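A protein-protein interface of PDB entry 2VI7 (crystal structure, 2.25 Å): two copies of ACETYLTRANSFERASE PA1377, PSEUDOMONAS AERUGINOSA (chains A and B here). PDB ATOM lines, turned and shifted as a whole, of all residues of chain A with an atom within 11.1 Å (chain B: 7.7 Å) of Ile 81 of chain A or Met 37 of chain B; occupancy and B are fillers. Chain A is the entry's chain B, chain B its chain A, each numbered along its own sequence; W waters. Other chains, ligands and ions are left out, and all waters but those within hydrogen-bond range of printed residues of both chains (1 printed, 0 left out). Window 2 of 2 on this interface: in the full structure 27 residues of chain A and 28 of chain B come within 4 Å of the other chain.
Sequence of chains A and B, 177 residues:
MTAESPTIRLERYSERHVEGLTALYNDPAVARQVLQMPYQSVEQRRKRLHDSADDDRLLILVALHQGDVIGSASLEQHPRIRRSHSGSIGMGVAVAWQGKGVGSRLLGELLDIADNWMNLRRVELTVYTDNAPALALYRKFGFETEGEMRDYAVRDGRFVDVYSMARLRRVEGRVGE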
ATOM      1  N   ARG A  57      10.622 -21.614  -6.613  1.00  0.00           N
ATOM      2  CA  ARG A  57      11.059 -21.368  -7.984  1.00  0.00           C
ATOM      3  C   ARG A  57      11.700 -22.630  -8.561  1.00  0.00           C
ATOM      4  O   ARG A  57      11.918 -22.730  -9.769  1.00  0.00           O
ATOM      5  CB  ARG A  57      12.036 -20.182  -8.054  1.00  0.00           C
ATOM      6  CG  ARG A  57      13.397 -20.410  -7.411  1.00  0.00           C
ATOM      7  CD  ARG A  57      14.345 -19.247  -7.716  1.00  0.00           C
ATOM      8  NE  ARG A  57      13.780 -17.952  -7.338  1.00  0.00           N
ATOM      9  CZ  ARG A  57      14.388 -17.062  -6.556  1.00  0.00           C
ATOM     10  NH1 ARG A  57      15.592 -17.319  -6.050  1.00  0.00           N
ATOM     11  NH2 ARG A  57      13.794 -15.902  -6.287  1.00  0.00           N
ATOM     12  N   GLU A  76      13.377 -24.962 -12.837  1.00  0.00           N
ATOM     13  CA  GLU A  76      13.872 -23.961 -11.915  1.00  0.00           C
ATOM     14  C   GLU A  76      13.918 -22.597 -12.581  1.00  0.00           C
ATOM     15  O   GLU A  76      14.605 -22.409 -13.583  1.00  0.00           O
ATOM     16  CB  GLU A  76      15.268 -24.322 -11.418  1.00  0.00           C
ATOM     17  CG  GLU A  76      15.750 -23.402 -10.306  1.00  0.00           C
ATOM     18  CD  GLU A  76      17.228 -23.566  -9.975  1.00  0.00           C
ATOM     19  OE1 GLU A  76      17.688 -24.723  -9.884  1.00  0.00           O
ATOM     20  OE2 GLU A  76      17.918 -22.536  -9.795  1.00  0.00           O
ATOM     21  N   GLN A  77      13.168 -21.645 -12.038  1.00  0.00           N
ATOM     22  CA  GLN A  77      13.162 -20.302 -12.587  1.00  0.00           C
ATOM     23  C   GLN A  77      14.521 -19.719 -12.238  1.00  0.00           C
ATOM     24  O   GLN A  77      15.022 -19.922 -11.135  1.00  0.00           O
ATOM     25  CB  GLN A  77      12.050 -19.481 -11.947  1.00  0.00           C
ATOM     26  CG  GLN A  77      12.004 -18.033 -12.370  1.00  0.00           C
ATOM     27  CD  GLN A  77      10.959 -17.258 -11.588  1.00  0.00           C
ATOM     28  OE1 GLN A  77      10.899 -17.349 -10.359  1.00  0.00           O
ATOM     29  NE2 GLN A  77      10.131 -16.491 -12.290  1.00  0.00           N
ATOM     30  N   HIS A  78      15.128 -19.005 -13.174  1.00  0.00           N
ATOM     31  CA  HIS A  78      16.437 -18.430 -12.919  1.00  0.00           C
ATOM     32  C   HIS A  78      16.377 -17.476 -11.735  1.00  0.00           C
ATOM     33  O   HIS A  78      15.463 -16.660 -11.636  1.00  0.00           O
ATOM     34  CB  HIS A  78      16.939 -17.693 -14.163  1.00  0.00           C
ATOM     35  CG  HIS A  78      18.428 -17.585 -14.231  1.00  0.00           C
ATOM     36  ND1 HIS A  78      19.163 -16.822 -13.349  1.00  0.00           N
ATOM     37  CD2 HIS A  78      19.327 -18.193 -15.041  1.00  0.00           C
ATOM     38  CE1 HIS A  78      20.450 -16.966 -13.611  1.00  0.00           C
ATOM     39  NE2 HIS A  78      20.577 -17.793 -14.634  1.00  0.00           N
ATOM     40  N   PRO A  79      17.348 -17.573 -10.813  1.00  0.00           N
ATOM     41  CA  PRO A  79      17.408 -16.711  -9.627  1.00  0.00           C
ATOM     42  C   PRO A  79      17.751 -15.238  -9.889  1.00  0.00           C
ATOM     43  O   PRO A  79      17.429 -14.373  -9.074  1.00  0.00           O
ATOM     44  CB  PRO A  79      18.445 -17.405  -8.755  1.00  0.00           C
ATOM     45  CG  PRO A  79      19.366 -18.020  -9.757  1.00  0.00           C
ATOM     46  CD  PRO A  79      18.391 -18.612 -10.753  1.00  0.00           C
ATOM     47  N   ARG A  80      18.405 -14.940 -11.008  1.00  0.00           N
ATOM     48  CA  ARG A  80      18.750 -13.550 -11.314  1.00  0.00           C
ATOM     49  C   ARG A  80      17.567 -12.808 -11.922  1.00  0.00           C
ATOM     50  O   ARG A  80      16.898 -13.304 -12.832  1.00  0.00           O
ATOM     51  CB  ARG A  80      19.947 -13.501 -12.251  1.00  0.00           C
ATOM     52  CG  ARG A  80      21.075 -14.342 -11.736  1.00  0.00           C
ATOM     53  CD  ARG A  80      22.305 -14.208 -12.574  1.00  0.00           C
ATOM     54  NE  ARG A  80      22.984 -12.953 -12.296  1.00  0.00           N
ATOM     55  CZ  ARG A  80      24.185 -12.645 -12.767  1.00  0.00           C
ATOM     56  NH1 ARG A  80      24.838 -13.510 -13.538  1.00  0.00           N
ATOM     57  NH2 ARG A  80      24.729 -11.470 -12.471  1.00  0.00           N
ATOM     58  N   ILE A  81      17.308 -11.611 -11.416  1.00  0.00           N
ATOM     59  CA  ILE A  81      16.170 -10.834 -11.884  1.00  0.00           C
ATOM     60  C   ILE A  81      16.110 -10.614 -13.397  1.00  0.00           C
ATOM     61  O   ILE A  81      15.040 -10.734 -14.007  1.00  0.00           O
ATOM     62  CB  ILE A  81      16.087  -9.473 -11.133  1.00  0.00           C
ATOM     63  CG1 ILE A  81      14.853  -8.692 -11.584  1.00  0.00           C
ATOM     64  CG2 ILE A  81      17.327  -8.668 -11.383  1.00  0.00           C
ATOM     65  CD1 ILE A  81      13.535  -9.444 -11.401  1.00  0.00           C
ATOM     66  N   ARG A  82      17.249 -10.317 -14.013  1.00  0.00           N
ATOM     67  CA  ARG A  82      17.263 -10.084 -15.454  1.00  0.00           C
ATOM     68  C   ARG A  82      17.141 -11.358 -16.290  1.00  0.00           C
ATOM     69  O   ARG A  82      17.078 -11.296 -17.511  1.00  0.00           O
ATOM     70  CB  ARG A  82      18.514  -9.287 -15.834  1.00  0.00           C
ATOM     71  CG  ARG A  82      18.538  -7.907 -15.192  1.00  0.00           C
ATOM     72  CD  ARG A  82      19.808  -7.148 -15.513  1.00  0.00           C
ATOM     73  NE  ARG A  82      19.955  -6.964 -16.950  1.00  0.00           N
ATOM     74  CZ  ARG A  82      21.042  -6.477 -17.531  1.00  0.00           C
ATOM     75  NH1 ARG A  82      21.078  -6.350 -18.849  1.00  0.00           N
ATOM     76  NH2 ARG A  82      22.092  -6.129 -16.797  1.00  0.00           N
ATOM     77  N   ARG A  83      17.074 -12.505 -15.621  1.00  0.00           N
ATOM     78  CA  ARG A  83      16.933 -13.794 -16.291  1.00  0.00           C
ATOM     79  C   ARG A  83      15.699 -14.531 -15.765  1.00  0.00           C
ATOM     80  O   ARG A  83      15.346 -15.605 -16.262  1.00  0.00           O
ATOM     81  CB  ARG A  83      18.182 -14.641 -16.042  1.00  0.00           C
ATOM     82  CG  ARG A  83      19.418 -14.192 -16.807  1.00  0.00           C
ATOM     83  CD  ARG A  83      19.433 -14.843 -18.169  1.00  0.00           C
ATOM     84  NE  ARG A  83      19.713 -16.274 -18.067  1.00  0.00           N
ATOM     85  CZ  ARG A  83      19.124 -17.224 -18.795  1.00  0.00           C
ATOM     86  NH1 ARG A  83      18.195 -16.925 -19.699  1.00  0.00           N
ATOM     87  NH2 ARG A  83      19.476 -18.489 -18.625  1.00  0.00           N
ATOM     88  N   SER A  84      15.030 -13.935 -14.779  1.00  0.00           N
ATOM     89  CA  SER A  84      13.857 -14.544 -14.139  1.00  0.00           C
ATOM     90  C   SER A  84      12.603 -14.785 -14.994  1.00  0.00           C
ATOM     91  O   SER A  84      11.622 -15.346 -14.506  1.00  0.00           O
ATOM     92  CB  SER A  84      13.483 -13.754 -12.875  1.00  0.00           C
ATOM     93  OG  SER A  84      13.157 -12.410 -13.175  1.00  0.00           O
ATOM     94  N   HIS A  85      12.630 -14.375 -16.256  1.00  0.00           N
ATOM     95  CA  HIS A  85      11.496 -14.607 -17.153  1.00  0.00           C
ATOM     96  C   HIS A  85      11.716 -15.984 -17.779  1.00  0.00           C
ATOM     97  O   HIS A  85      10.875 -16.488 -18.530  1.00  0.00           O
ATOM     98  CB  HIS A  85      11.453 -13.545 -18.262  1.00  0.00           C
ATOM     99  CG  HIS A  85      12.713 -13.471 -19.066  1.00  0.00           C
ATOM    100  ND1 HIS A  85      13.896 -12.991 -18.547  1.00  0.00           N
ATOM    101  CD2 HIS A  85      13.001 -13.909 -20.316  1.00  0.00           C
ATOM    102  CE1 HIS A  85      14.859 -13.143 -19.437  1.00  0.00           C
ATOM    103  NE2 HIS A  85      14.343 -13.697 -20.519  1.00  0.00           N
ATOM    104  N   SER A  86      12.863 -16.582 -17.461  1.00  0.00           N
ATOM    105  CA  SER A  86      13.213 -17.895 -17.988  1.00  0.00           C
ATOM    106  C   SER A  86      13.377 -18.952 -16.902  1.00  0.00           C
ATOM    107  O   SER A  86      13.637 -18.653 -15.739  1.00  0.00           O
ATOM    108  CB  SER A  86      14.508 -17.814 -18.807  1.00  0.00           C
ATOM    109  OG  SER A  86      15.635 -17.706 -17.958  1.00  0.00           O
ATOM    110  N   GLY A  87      13.213 -20.201 -17.313  1.00  0.00           N
ATOM    111  CA  GLY A  87      13.367 -21.318 -16.411  1.00  0.00           C
ATOM    112  C   GLY A  87      14.133 -22.395 -17.154  1.00  0.00           C
ATOM    113  O   GLY A  87      14.184 -22.396 -18.385  1.00  0.00           O
ATOM    114  N   ASN A 119       4.258 -18.211 -15.339  1.00  0.00           N
ATOM    115  CA  ASN A 119       4.154 -17.289 -16.460  1.00  0.00           C
ATOM    116  C   ASN A 119       5.527 -17.000 -17.082  1.00  0.00           C
ATOM    117  O   ASN A 119       5.861 -15.850 -17.380  1.00  0.00           O
ATOM    118  CB  ASN A 119       3.469 -15.990 -15.995  1.00  0.00           C
ATOM    119  CG  ASN A 119       3.084 -15.071 -17.154  1.00  0.00           C
ATOM    120  OD1 ASN A 119       2.397 -15.481 -18.088  1.00  0.00           O
ATOM    121  ND2 ASN A 119       3.517 -13.819 -17.083  1.00  0.00           N
ATOM    122  N   LEU A 120       6.321 -18.052 -17.277  1.00  0.00           N
ATOM    123  CA  LEU A 120       7.650 -17.902 -17.864  1.00  0.00           C
ATOM    124  C   LEU A 120       7.585 -17.665 -19.368  1.00  0.00           C
ATOM    125  O   LEU A 120       6.721 -18.208 -20.053  1.00  0.00           O
ATOM    126  CB  LEU A 120       8.490 -19.147 -17.590  1.00  0.00           C
ATOM    127  CG  LEU A 120       8.811 -19.482 -16.134  1.00  0.00           C
ATOM    128  CD1 LEU A 120       9.484 -20.850 -16.076  1.00  0.00           C
ATOM    129  CD2 LEU A 120       9.700 -18.399 -15.524  1.00  0.00           C
ATOM    130  N   ARG A 121       8.502 -16.850 -19.880  1.00  0.00           N
ATOM    131  CA  ARG A 121       8.561 -16.554 -21.313  1.00  0.00           C
ATOM    132  C   ARG A 121       9.477 -17.544 -22.040  1.00  0.00           C
ATOM    133  O   ARG A 121       9.275 -17.852 -23.214  1.00  0.00           O
ATOM    134  CB  ARG A 121       9.075 -15.117 -21.533  1.00  0.00           C
ATOM    135  CG  ARG A 121       9.583 -14.762 -22.946  1.00  0.00           C
ATOM    136  CD  ARG A 121       8.490 -14.689 -24.003  1.00  0.00           C
ATOM    137  NE  ARG A 121       9.026 -14.303 -25.312  1.00  0.00           N
ATOM    138  CZ  ARG A 121       8.453 -14.579 -26.490  1.00  0.00           C
ATOM    139  NH1 ARG A 121       7.307 -15.257 -26.548  1.00  0.00           N
ATOM    140  NH2 ARG A 121       9.026 -14.166 -27.621  1.00  0.00           N
ATOM    141  N   THR B  22      31.727  -2.316  -6.795  1.00  0.00           N
ATOM    142  CA  THR B  22      30.335  -1.915  -6.678  1.00  0.00           C
ATOM    143  C   THR B  22      30.078  -0.687  -7.543  1.00  0.00           C
ATOM    144  O   THR B  22      29.063  -0.600  -8.231  1.00  0.00           O
ATOM    145  CB  THR B  22      30.001  -1.587  -5.228  1.00  0.00           C
ATOM    146  OG1 THR B  22      30.186  -2.757  -4.428  1.00  0.00           O
ATOM    147  CG2 THR B  22      28.577  -1.169  -5.102  1.00  0.00           C
ATOM    148  N   TYR B  25      29.808  -1.529 -11.396  1.00  0.00           N
ATOM    149  CA  TYR B  25      28.503  -1.996 -11.828  1.00  0.00           C
ATOM    150  C   TYR B  25      27.397  -0.957 -11.684  1.00  0.00           C
ATOM    151  O   TYR B  25      26.316  -1.117 -12.253  1.00  0.00           O
ATOM    152  CB  TYR B  25      28.154  -3.271 -11.062  1.00  0.00           C
ATOM    153  CG  TYR B  25      29.044  -4.437 -11.441  1.00  0.00           C
ATOM    154  CD1 TYR B  25      29.408  -5.402 -10.501  1.00  0.00           C
ATOM    155  CD2 TYR B  25      29.518  -4.578 -12.749  1.00  0.00           C
ATOM    156  CE1 TYR B  25      30.228  -6.482 -10.855  1.00  0.00           C
ATOM    157  CE2 TYR B  25      30.332  -5.646 -13.114  1.00  0.00           C
ATOM    158  CZ  TYR B  25      30.683  -6.596 -12.164  1.00  0.00           C
ATOM    159  OH  TYR B  25      31.472  -7.666 -12.524  1.00  0.00           O
ATOM    160  N   ASN B  26      27.666   0.110 -10.932  1.00  0.00           N
ATOM    161  CA  ASN B  26      26.676   1.163 -10.753  1.00  0.00           C
ATOM    162  C   ASN B  26      26.625   2.058 -11.986  1.00  0.00           C
ATOM    163  O   ASN B  26      25.785   2.946 -12.073  1.00  0.00           O
ATOM    164  CB  ASN B  26      26.963   1.987  -9.487  1.00  0.00           C
ATOM    165  CG  ASN B  26      26.390   1.344  -8.223  1.00  0.00           C
ATOM    166  OD1 ASN B  26      25.902   0.206  -8.247  1.00  0.00           O
ATOM    167  ND2 ASN B  26      26.453   2.069  -7.110  1.00  0.00           N
ATOM    168  N   ASP B  27      27.530   1.829 -12.934  1.00  0.00           N
ATOM    169  CA  ASP B  27      27.517   2.589 -14.180  1.00  0.00           C
ATOM    170  C   ASP B  27      26.605   1.765 -15.090  1.00  0.00           C
ATOM    171  O   ASP B  27      26.951   0.649 -15.478  1.00  0.00           O
ATOM    172  CB  ASP B  27      28.920   2.684 -14.794  1.00  0.00           C
ATOM    173  CG  ASP B  27      28.940   3.478 -16.108  1.00  0.00           C
ATOM    174  OD1 ASP B  27      27.857   3.705 -16.696  1.00  0.00           O
ATOM    175  OD2 ASP B  27      30.043   3.864 -16.559  1.00  0.00           O
ATOM    176  N   ALA B  31      26.826  -2.104 -16.440  1.00  0.00           N
ATOM    177  CA  ALA B  31      25.859  -3.086 -15.976  1.00  0.00           C
ATOM    178  C   ALA B  31      24.942  -3.624 -17.071  1.00  0.00           C
ATOM    179  O   ALA B  31      24.589  -4.802 -17.057  1.00  0.00           O
ATOM    180  CB  ALA B  31      25.020  -2.491 -14.846  1.00  0.00           C
ATOM    181  N   ARG B  32      24.569  -2.786 -18.033  1.00  0.00           N
ATOM    182  CA  ARG B  32      23.646  -3.238 -19.067  1.00  0.00           C
ATOM    183  C   ARG B  32      24.202  -4.239 -20.059  1.00  0.00           C
ATOM    184  O   ARG B  32      23.436  -4.961 -20.682  1.00  0.00           O
ATOM    185  CB  ARG B  32      23.040  -2.047 -19.814  1.00  0.00           C
ATOM    186  CG  ARG B  32      23.991  -1.298 -20.700  1.00  0.00           C
ATOM    187  CD  ARG B  32      23.304  -0.120 -21.375  1.00  0.00           C
ATOM    188  NE  ARG B  32      22.481  -0.513 -22.520  1.00  0.00           N
ATOM    189  CZ  ARG B  32      22.965  -0.966 -23.679  1.00  0.00           C
ATOM    190  NH1 ARG B  32      24.275  -1.095 -23.854  1.00  0.00           N
ATOM    191  NH2 ARG B  32      22.140  -1.265 -24.679  1.00  0.00           N
ATOM    192  N   VAL B  34      26.077  -6.775 -19.256  1.00  0.00           N
ATOM    193  CA  VAL B  34      26.247  -8.028 -18.521  1.00  0.00           C
ATOM    194  C   VAL B  34      24.869  -8.330 -17.911  1.00  0.00           C
ATOM    195  O   VAL B  34      23.848  -7.947 -18.494  1.00  0.00           O
ATOM    196  CB  VAL B  34      27.366  -7.932 -17.416  1.00  0.00           C
ATOM    197  CG1 VAL B  34      28.737  -7.889 -18.077  1.00  0.00           C
ATOM    198  CG2 VAL B  34      27.191  -6.695 -16.561  1.00  0.00           C
ATOM    199  N   LEU B  35      24.815  -9.008 -16.770  1.00  0.00           N
ATOM    200  CA  LEU B  35      23.525  -9.324 -16.150  1.00  0.00           C
ATOM    201  C   LEU B  35      23.371  -8.728 -14.756  1.00  0.00           C
ATOM    202  O   LEU B  35      22.427  -9.053 -14.034  1.00  0.00           O
ATOM    203  CB  LEU B  35      23.315 -10.841 -16.090  1.00  0.00           C
ATOM    204  CG  LEU B  35      23.011 -11.580 -17.395  1.00  0.00           C
ATOM    205  CD1 LEU B  35      23.085 -13.091 -17.199  1.00  0.00           C
ATOM    206  CD2 LEU B  35      21.645 -11.162 -17.868  1.00  0.00           C
ATOM    207  N   GLN B  36      24.303  -7.850 -14.395  1.00  0.00           N
ATOM    208  CA  GLN B  36      24.303  -7.180 -13.098  1.00  0.00           C
ATOM    209  C   GLN B  36      23.192  -6.141 -12.978  1.00  0.00           C
ATOM    210  O   GLN B  36      22.665  -5.646 -13.977  1.00  0.00           O
ATOM    211  CB  GLN B  36      25.638  -6.464 -12.862  1.00  0.00           C
ATOM    212  CG  GLN B  36      26.863  -7.345 -12.802  1.00  0.00           C
ATOM    213  CD  GLN B  36      26.877  -8.229 -11.585  1.00  0.00           C
ATOM    214  OE1 GLN B  36      26.469  -7.814 -10.493  1.00  0.00           O
ATOM    215  NE2 GLN B  36      27.364  -9.452 -11.753  1.00  0.00           N
ATOM    216  N   MET B  37      22.860  -5.806 -11.735  1.00  0.00           N
ATOM    217  CA  MET B  37      21.844  -4.809 -11.430  1.00  0.00           C
ATOM    218  C   MET B  37      22.536  -3.569 -10.867  1.00  0.00           C
ATOM    219  O   MET B  37      23.550  -3.682 -10.170  1.00  0.00           O
ATOM    220  CB  MET B  37      20.850  -5.358 -10.393  1.00  0.00           C
ATOM    221  CG  MET B  37      19.856  -6.384 -10.928  1.00  0.00           C
ATOM    222  SD  MET B  37      18.677  -5.666 -12.104  1.00  0.00           S
ATOM    223  CE  MET B  37      17.382  -5.149 -10.999  1.00  0.00           C
ATOM    224  N   PRO B  38      22.021  -2.366 -11.183  1.00  0.00           N
ATOM    225  CA  PRO B  38      22.672  -1.172 -10.640  1.00  0.00           C
ATOM    226  C   PRO B  38      22.311  -0.970  -9.168  1.00  0.00           C
ATOM    227  O   PRO B  38      21.568  -1.765  -8.583  1.00  0.00           O
ATOM    228  CB  PRO B  38      22.153  -0.051 -11.547  1.00  0.00           C
ATOM    229  CG  PRO B  38      20.790  -0.524 -11.914  1.00  0.00           C
ATOM    230  CD  PRO B  38      20.997  -2.000 -12.182  1.00  0.00           C
ATOM    231  N   TYR B  39      22.847   0.091  -8.577  1.00  0.00           N
ATOM    232  CA  TYR B  39      22.582   0.402  -7.178  1.00  0.00           C
ATOM    233  C   TYR B  39      22.823  -0.750  -6.220  1.00  0.00           C
ATOM    234  O   TYR B  39      22.045  -0.966  -5.284  1.00  0.00           O
ATOM    235  CB  TYR B  39      21.151   0.921  -6.991  1.00  0.00           C
ATOM    236  CG  TYR B  39      20.968   2.311  -7.531  1.00  0.00           C
ATOM    237  CD1 TYR B  39      21.718   3.372  -7.035  1.00  0.00           C
ATOM    238  CD2 TYR B  39      20.097   2.557  -8.589  1.00  0.00           C
ATOM    239  CE1 TYR B  39      21.614   4.639  -7.585  1.00  0.00           C
ATOM    240  CE2 TYR B  39      19.985   3.823  -9.148  1.00  0.00           C
ATOM    241  CZ  TYR B  39      20.750   4.857  -8.644  1.00  0.00           C
ATOM    242  OH  TYR B  39      20.675   6.103  -9.222  1.00  0.00           O
ATOM    243  N   GLN B  40      23.890  -1.501  -6.459  1.00  0.00           N
ATOM    244  CA  GLN B  40      24.244  -2.578  -5.554  1.00  0.00           C
ATOM    245  C   GLN B  40      24.973  -1.855  -4.419  1.00  0.00           C
ATOM    246  O   GLN B  40      25.518  -0.754  -4.618  1.00  0.00           O
ATOM    247  CB  GLN B  40      25.171  -3.595  -6.237  1.00  0.00           C
ATOM    248  CG  GLN B  40      24.452  -4.647  -7.073  1.00  0.00           C
ATOM    249  CD  GLN B  40      25.408  -5.491  -7.902  1.00  0.00           C
ATOM    250  N   SER B  41      24.968  -2.449  -3.233  1.00  0.00           N
ATOM    251  CA  SER B  41      25.629  -1.833  -2.092  1.00  0.00           C
ATOM    252  C   SER B  41      26.786  -2.682  -1.585  1.00  0.00           C
ATOM    253  O   SER B  41      26.713  -3.924  -1.547  1.00  0.00           O
ATOM    254  N   ARG B  45      27.600  -7.524  -1.127  1.00  0.00           N
ATOM    255  CA  ARG B  45      28.764  -8.095  -1.799  1.00  0.00           C
ATOM    256  C   ARG B  45      29.732  -8.706  -0.797  1.00  0.00           C
ATOM    257  O   ARG B  45      30.178  -9.844  -0.960  1.00  0.00           O
ATOM    258  CB  ARG B  45      29.479  -7.024  -2.628  1.00  0.00           C
ATOM    259  CG  ARG B  45      28.669  -6.602  -3.835  1.00  0.00           C
ATOM    260  CD  ARG B  45      29.483  -5.840  -4.875  1.00  0.00           C
ATOM    261  NE  ARG B  45      28.852  -5.949  -6.192  1.00  0.00           N
ATOM    262  CZ  ARG B  45      28.909  -7.030  -6.974  1.00  0.00           C
ATOM    263  NH1 ARG B  45      29.581  -8.113  -6.588  1.00  0.00           N
ATOM    264  NH2 ARG B  45      28.272  -7.031  -8.142  1.00  0.00           N
ATOM    265  N   ALA B 153      17.793 -12.449 -21.882  1.00  0.00           N
ATOM    266  CA  ALA B 153      17.802 -11.583 -20.712  1.00  0.00           C
ATOM    267  C   ALA B 153      17.121 -10.256 -20.971  1.00  0.00           C
ATOM    268  O   ALA B 153      16.768  -9.932 -22.101  1.00  0.00           O
ATOM    269  CB  ALA B 153      19.247 -11.333 -20.254  1.00  0.00           C
ATOM    270  N   VAL B 154      16.934  -9.499 -19.896  1.00  0.00           N
ATOM    271  CA  VAL B 154      16.324  -8.180 -19.956  1.00  0.00           C
ATOM    272  C   VAL B 154      17.456  -7.155 -20.026  1.00  0.00           C
ATOM    273  O   VAL B 154      18.479  -7.285 -19.347  1.00  0.00           O
ATOM    274  CB  VAL B 154      15.468  -7.880 -18.679  1.00  0.00           C
ATOM    275  CG1 VAL B 154      14.891  -6.467 -18.739  1.00  0.00           C
ATOM    276  CG2 VAL B 154      14.353  -8.882 -18.549  1.00  0.00           C
ATOM    277  N   PHE B 159      13.468  -7.777 -23.857  1.00  0.00           N
ATOM    278  CA  PHE B 159      14.184  -9.042 -23.946  1.00  0.00           C
ATOM    279  C   PHE B 159      15.119  -8.987 -25.145  1.00  0.00           C
ATOM    280  O   PHE B 159      14.711  -8.650 -26.255  1.00  0.00           O
ATOM    281  CB  PHE B 159      13.189 -10.184 -24.081  1.00  0.00           C
ATOM    282  CG  PHE B 159      12.360 -10.399 -22.858  1.00  0.00           C
ATOM    283  CD1 PHE B 159      11.016 -10.722 -22.970  1.00  0.00           C
ATOM    284  CD2 PHE B 159      12.921 -10.254 -21.591  1.00  0.00           C
ATOM    285  CE1 PHE B 159      10.247 -10.926 -21.846  1.00  0.00           C
ATOM    286  CE2 PHE B 159      12.168 -10.456 -20.457  1.00  0.00           C
ATOM    287  CZ  PHE B 159      10.822 -10.781 -20.580  1.00  0.00           C
HETATM  288  O   HOH W   1      19.931  -9.713 -12.980  1.00  0.00           O
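Water W1 bridges the backbone carbonyl oxygen of Leu 35 of chain B (2.8 Å) and the backbone NH of Arg 82 of chain A (2.9 Å).
Met 37 of chain B touches two residues of chain A.
Of the printed residues of chain A, Gln 36 of chain B touches Arg 80 and Arg 82.
No residue of chain A comes within 4 Å of Pro 38 of chain B.
Gln 40 of chain B touches none of the printed residues of chain A.
Of the printed residues of chain A, Leu 35 of chain B touches Arg 80 (3.7 Å), Arg 82 (3.5 Å) and Arg 83 (3.8 Å).
Of the printed residues of chain A, Ala 31 of chain B touches Arg 82 (2.8 Å).
Asp 27 of chain B touches none of the printed residues of chain A.
The nearest residue of chain A that does not touch Met 37 of chain B is Arg 80 of chain A (6.0 Å).
The nearest printed residue of chain A that does not touch Ala 153 of chain B is Arg 83 of chain A (4.1 Å).
Hydrophobic or aromatic side chains of chain A within 4 Å of the printed part of chain B: Ile 81 and His 85.
Hydrophobic or aromatic side chains of chain B that line the printed part of chain A: Leu 35, Met 37, Ala 153, Val 154 and Phe 159.
Among the printed residues, 14 pairs touch across the chains.
Among the printed residues, no Asp or Glu carboxylate lies within 4 Å of a Lys or Arg side-chain nitrogen of the other chain.
Among the printed residues, merely in contact across the chains: Arg 82 of chain A with Ala 153 of chain B (3.3 Å), His 85 of chain A with Phe 159 of chain B (3.4 Å), Ile 81 of chain A with Met 37 of chain B (3.4 Å), Arg 82 of chain A with Leu 35 of chain B (3.5 Å), His 85 of chain A with Ala 153 of chain B (3.6 Å), Arg 80 of chain A with Leu 35 of chain B (3.7 Å), Arg 82 of chain A with Met 37 of chain B (3.8 Å) and Arg 83 of chain A with Leu 35 of chain B (3.8 Å).
The backbone carbonyl oxygen of Ala 31 of chain B lies within hydrogen-bond range of the guanidinium group of Arg 82 of chain A, at 2.8 Å.
The backbone carbonyl oxygen of Arg 32 of chain B sits at hydrogen-bond distance from the guanidinium group of Arg 82 of chain A (3.3 Å).
The backbone carbonyl oxygen (O) of Val 34 of chain B sits at hydrogen-bond distance from the guanidinium group (NH2) of Arg 82 of chain A, at 3.0 Å.
The side-chain amide nitrogen (NE2) of Gln 36 of chain B sits close to the guanidinium group (NH2) of Arg 80 of chain A (3.4 Å).
The backbone carbonyl oxygen (O) of Gln 36 of chain B sits at hydrogen-bond distance from the guanidinium group (NH2) of Arg 82 of chain A (2.9 Å).
O of Val 154 of chain B lies within hydrogen-bond range of NH1 of Arg 82 of chain A (2.8 Å).
The side-chain amide oxygen (OE1) of Gln 36 of chain B lies within hydrogen-bond range of the guanidinium group (NH2) of Arg 45 of chain B (3.1 Å).
N of Arg 80 of chain A is in hydrogen-bond range of ND1 of His 78 of chain A (3.1 Å).
O of Ile 81 of chain A is in hydrogen-bond range of OG of Ser 84 of chain A.
The backbone carbonyl oxygen (O) of Arg 83 of chain A is in hydrogen-bond range of the side-chain hydroxyl (OG) of Ser 86 of chain A, at 2.7 Å.
The backbone carbonyl oxygen (O) of His 85 of chain A lies within hydrogen-bond range of the backbone NH (N) of Arg 121 of chain A, 2.8 Å away.
No position is printed for both chains.
Of the 14 pairs that touch across the chains among the printed residues, none has its exchanged pair printed and touching as well.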
